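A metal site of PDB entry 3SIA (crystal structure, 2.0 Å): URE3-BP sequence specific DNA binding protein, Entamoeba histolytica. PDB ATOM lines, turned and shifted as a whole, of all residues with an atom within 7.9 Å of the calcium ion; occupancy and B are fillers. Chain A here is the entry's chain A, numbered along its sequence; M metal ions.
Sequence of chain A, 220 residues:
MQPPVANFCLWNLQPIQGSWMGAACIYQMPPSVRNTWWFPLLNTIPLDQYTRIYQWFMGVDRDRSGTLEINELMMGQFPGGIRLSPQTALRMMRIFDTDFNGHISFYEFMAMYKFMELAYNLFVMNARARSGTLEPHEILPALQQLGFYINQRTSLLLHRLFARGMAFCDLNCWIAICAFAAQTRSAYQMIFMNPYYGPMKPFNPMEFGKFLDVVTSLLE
The backbone NH (N) of Arg 64 lies close to the side-chain carboxylate (OD1) of Asp 61 (3.3 Å). OD2 of Asp 61 sits at hydrogen-bond distance from N of Gly 66, at 2.8 Å. The side-chain carboxylate (OE2) of Glu 69 is in hydrogen-bond range of a ring nitrogen (ND1) of His 103 (2.6 Å). The side-chain carboxylate (OE2) of Glu 72 sits close to the backbone NH (N) of Arg 62, at 3.2 Å.
The calcium ion is bound by O of Thr 67 (2.2 Å), OD1 of Asp 61 (2.3 Å), OD1 of Asp 63 (2.4 Å), OE1 of Glu 69 (2.5 Å), OG of Ser 65 (2.5 Å), OE2 of Glu 72 (2.6 Å) and OE1 of Glu 72 (2.6 Å).
Within 4 Å of the calcium ion: Asp 61, Asp 63, Ser 65, Thr 67, Glu 69 and Glu 72.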
ATOM      1  N   PHE A  57     -25.595  20.216 -22.876  1.00  0.00           N
ATOM      2  CA  PHE A  57     -25.779  18.855 -23.394  1.00  0.00           C
ATOM      3  C   PHE A  57     -24.915  18.643 -24.636  1.00  0.00           C
ATOM      4  O   PHE A  57     -24.239  17.658 -24.732  1.00  0.00           O
ATOM      5  CB  PHE A  57     -27.253  18.666 -23.762  1.00  0.00           C
ATOM      6  CG  PHE A  57     -27.626  17.274 -24.202  1.00  0.00           C
ATOM      7  CD1 PHE A  57     -27.797  16.244 -23.286  1.00  0.00           C
ATOM      8  CD2 PHE A  57     -27.921  17.025 -25.549  1.00  0.00           C
ATOM      9  CE1 PHE A  57     -28.231  14.961 -23.718  1.00  0.00           C
ATOM     10  CE2 PHE A  57     -28.326  15.763 -25.969  1.00  0.00           C
ATOM     11  CZ  PHE A  57     -28.462  14.727 -25.032  1.00  0.00           C
ATOM     12  N   VAL A  60     -21.296  18.121 -23.770  1.00  0.00           N
ATOM     13  CA  VAL A  60     -20.953  16.819 -23.221  1.00  0.00           C
ATOM     14  C   VAL A  60     -21.107  15.665 -24.271  1.00  0.00           C
ATOM     15  O   VAL A  60     -20.361  14.705 -24.275  1.00  0.00           O
ATOM     16  CB  VAL A  60     -21.837  16.541 -21.975  1.00  0.00           C
ATOM     17  CG1 VAL A  60     -21.448  15.225 -21.340  1.00  0.00           C
ATOM     18  CG2 VAL A  60     -21.708  17.716 -21.006  1.00  0.00           C
ATOM     19  N   ASP A  61     -22.085  15.787 -25.156  1.00  0.00           N
ATOM     20  CA  ASP A  61     -22.327  14.810 -26.229  1.00  0.00           C
ATOM     21  C   ASP A  61     -21.240  14.862 -27.357  1.00  0.00           C
ATOM     22  O   ASP A  61     -21.475  15.380 -28.488  1.00  0.00           O
ATOM     23  CB  ASP A  61     -23.727  15.057 -26.799  1.00  0.00           C
ATOM     24  CG  ASP A  61     -24.113  14.072 -27.891  1.00  0.00           C
ATOM     25  OD1 ASP A  61     -23.473  13.016 -28.044  1.00  0.00           O
ATOM     26  OD2 ASP A  61     -25.055  14.380 -28.632  1.00  0.00           O
ATOM     27  N   ARG A  62     -20.106  14.248 -27.054  1.00  0.00           N
ATOM     28  CA  ARG A  62     -18.953  14.237 -27.931  1.00  0.00           C
ATOM     29  C   ARG A  62     -19.150  13.556 -29.313  1.00  0.00           C
ATOM     30  O   ARG A  62     -18.479  13.944 -30.242  1.00  0.00           O
ATOM     31  CB  ARG A  62     -17.740  13.600 -27.168  1.00  0.00           C
ATOM     32  N   ASP A  63     -20.021  12.566 -29.465  1.00  0.00           N
ATOM     33  CA  ASP A  63     -20.275  11.954 -30.794  1.00  0.00           C
ATOM     34  C   ASP A  63     -21.553  12.463 -31.538  1.00  0.00           C
ATOM     35  O   ASP A  63     -21.967  11.900 -32.543  1.00  0.00           O
ATOM     36  CB  ASP A  63     -20.256  10.419 -30.681  1.00  0.00           C
ATOM     37  CG  ASP A  63     -21.334   9.864 -29.802  1.00  0.00           C
ATOM     38  OD1 ASP A  63     -22.134  10.651 -29.245  1.00  0.00           O
ATOM     39  OD2 ASP A  63     -21.392   8.624 -29.692  1.00  0.00           O
ATOM     40  N   ARG A  64     -22.133  13.565 -31.033  1.00  0.00           N
ATOM     41  CA  ARG A  64     -23.369  14.180 -31.552  1.00  0.00           C
ATOM     42  C   ARG A  64     -24.533  13.180 -31.754  1.00  0.00           C
ATOM     43  O   ARG A  64     -25.314  13.313 -32.679  1.00  0.00           O
ATOM     44  CB  ARG A  64     -23.085  14.967 -32.795  1.00  0.00           C
ATOM     45  CG  ARG A  64     -21.920  15.987 -32.632  1.00  0.00           C
ATOM     46  CD  ARG A  64     -21.730  16.868 -33.911  1.00  0.00           C
ATOM     47  NE  ARG A  64     -23.044  17.327 -34.391  1.00  0.00           N
ATOM     48  CZ  ARG A  64     -23.538  17.136 -35.616  1.00  0.00           C
ATOM     49  NH1 ARG A  64     -22.839  16.542 -36.563  1.00  0.00           N
ATOM     50  NH2 ARG A  64     -24.761  17.589 -35.888  1.00  0.00           N
ATOM     51  N   SER A  65     -24.623  12.174 -30.884  1.00  0.00           N
ATOM     52  CA  SER A  65     -25.682  11.174 -30.998  1.00  0.00           C
ATOM     53  C   SER A  65     -27.035  11.692 -30.497  1.00  0.00           C
ATOM     54  O   SER A  65     -28.076  11.062 -30.710  1.00  0.00           O
ATOM     55  CB  SER A  65     -25.334   9.907 -30.217  1.00  0.00           C
ATOM     56  OG  SER A  65     -25.299  10.155 -28.819  1.00  0.00           O
ATOM     57  N   GLY A  66     -27.035  12.832 -29.835  1.00  0.00           N
ATOM     58  CA  GLY A  66     -28.305  13.320 -29.287  1.00  0.00           C
ATOM     59  C   GLY A  66     -28.567  12.647 -27.948  1.00  0.00           C
ATOM     60  O   GLY A  66     -29.681  12.734 -27.420  1.00  0.00           O
ATOM     61  N   THR A  67     -27.544  11.956 -27.440  1.00  0.00           N
ATOM     62  CA  THR A  67     -27.628  11.265 -26.182  1.00  0.00           C
ATOM     63  C   THR A  67     -26.286  11.274 -25.454  1.00  0.00           C
ATOM     64  O   THR A  67     -25.231  11.453 -26.050  1.00  0.00           O
ATOM     65  CB  THR A  67     -28.107   9.808 -26.358  1.00  0.00           C
ATOM     66  OG1 THR A  67     -27.154   9.064 -27.090  1.00  0.00           O
ATOM     67  CG2 THR A  67     -29.456   9.737 -27.074  1.00  0.00           C
ATOM     68  N   LEU A  68     -26.333  11.053 -24.173  1.00  0.00           N
ATOM     69  CA  LEU A  68     -25.094  10.952 -23.377  1.00  0.00           C
ATOM     70  C   LEU A  68     -24.869   9.509 -22.908  1.00  0.00           C
ATOM     71  O   LEU A  68     -25.749   8.855 -22.370  1.00  0.00           O
ATOM     72  CB  LEU A  68     -25.136  11.894 -22.176  1.00  0.00           C
ATOM     73  CG  LEU A  68     -25.387  13.374 -22.486  1.00  0.00           C
ATOM     74  CD1 LEU A  68     -25.344  14.200 -21.206  1.00  0.00           C
ATOM     75  CD2 LEU A  68     -24.446  13.977 -23.541  1.00  0.00           C
ATOM     76  N   GLU A  69     -23.650   9.044 -23.121  1.00  0.00           N
ATOM     77  CA  GLU A  69     -23.224   7.749 -22.707  1.00  0.00           C
ATOM     78  C   GLU A  69     -22.293   7.877 -21.524  1.00  0.00           C
ATOM     79  O   GLU A  69     -21.837   8.969 -21.197  1.00  0.00           O
ATOM     80  CB  GLU A  69     -22.508   7.059 -23.887  1.00  0.00           C
ATOM     81  CG  GLU A  69     -23.472   6.595 -24.951  1.00  0.00           C
ATOM     82  CD  GLU A  69     -24.160   7.746 -25.677  1.00  0.00           C
ATOM     83  OE1 GLU A  69     -23.435   8.565 -26.293  1.00  0.00           O
ATOM     84  OE2 GLU A  69     -25.425   7.801 -25.689  1.00  0.00           O
ATOM     85  N   ILE A  70     -21.974   6.773 -20.883  1.00  0.00           N
ATOM     86  CA  ILE A  70     -21.237   6.855 -19.606  1.00  0.00           C
ATOM     87  C   ILE A  70     -19.842   7.485 -19.801  1.00  0.00           C
ATOM     88  O   ILE A  70     -19.404   8.330 -18.971  1.00  0.00           O
ATOM     89  CB  ILE A  70     -21.121   5.486 -18.932  1.00  0.00           C
ATOM     90  CG1 ILE A  70     -20.478   5.653 -17.560  1.00  0.00           C
ATOM     91  CG2 ILE A  70     -20.429   4.427 -19.906  1.00  0.00           C
ATOM     92  CD1 ILE A  70     -20.657   4.463 -16.694  1.00  0.00           C
ATOM     93  N   GLU A  72     -19.067   9.758 -21.919  1.00  0.00           N
ATOM     94  CA  GLU A  72     -19.296  11.231 -22.006  1.00  0.00           C
ATOM     95  C   GLU A  72     -19.520  11.891 -20.649  1.00  0.00           C
ATOM     96  O   GLU A  72     -19.067  13.037 -20.415  1.00  0.00           O
ATOM     97  CB  GLU A  72     -20.432  11.574 -22.989  1.00  0.00           C
ATOM     98  CG  GLU A  72     -20.038  11.250 -24.434  1.00  0.00           C
ATOM     99  CD  GLU A  72     -21.202  11.163 -25.392  1.00  0.00           C
ATOM    100  OE1 GLU A  72     -22.350  11.061 -24.922  1.00  0.00           O
ATOM    101  OE2 GLU A  72     -20.978  11.176 -26.645  1.00  0.00           O
ATOM    102  N   HIS A 103     -28.184   5.023 -22.420  1.00  0.00           N
ATOM    103  CA  HIS A 103     -28.165   6.390 -22.933  1.00  0.00           C
ATOM    104  C   HIS A 103     -28.944   7.304 -21.976  1.00  0.00           C
ATOM    105  O   HIS A 103     -29.967   6.887 -21.405  1.00  0.00           O
ATOM    106  CB  HIS A 103     -28.819   6.447 -24.308  1.00  0.00           C
ATOM    107  CG  HIS A 103     -28.208   5.524 -25.303  1.00  0.00           C
ATOM    108  ND1 HIS A 103     -26.918   5.695 -25.765  1.00  0.00           N
ATOM    109  CD2 HIS A 103     -28.674   4.406 -25.896  1.00  0.00           C
ATOM    110  CE1 HIS A 103     -26.618   4.703 -26.586  1.00  0.00           C
ATOM    111  NE2 HIS A 103     -27.665   3.914 -26.690  1.00  0.00           N
ATOM    112  N   ILE A 104     -28.475   8.528 -21.813  1.00  0.00           N
ATOM    113  CA  ILE A 104     -29.267   9.586 -21.192  1.00  0.00           C
ATOM    114  C   ILE A 104     -29.783  10.498 -22.335  1.00  0.00           C
ATOM    115  O   ILE A 104     -29.001  11.099 -23.060  1.00  0.00           O
ATOM    116  CB  ILE A 104     -28.384  10.359 -20.147  1.00  0.00           C
ATOM    117  CG1 ILE A 104     -28.360   9.557 -18.847  1.00  0.00           C
ATOM    118  CG2 ILE A 104     -28.924  11.801 -19.849  1.00  0.00           C
ATOM    119  CD1 ILE A 104     -27.379  10.095 -17.928  1.00  0.00           C
HETATM  120 CA    CA M   1     -23.438  10.853 -27.266  1.00  0.00          CA
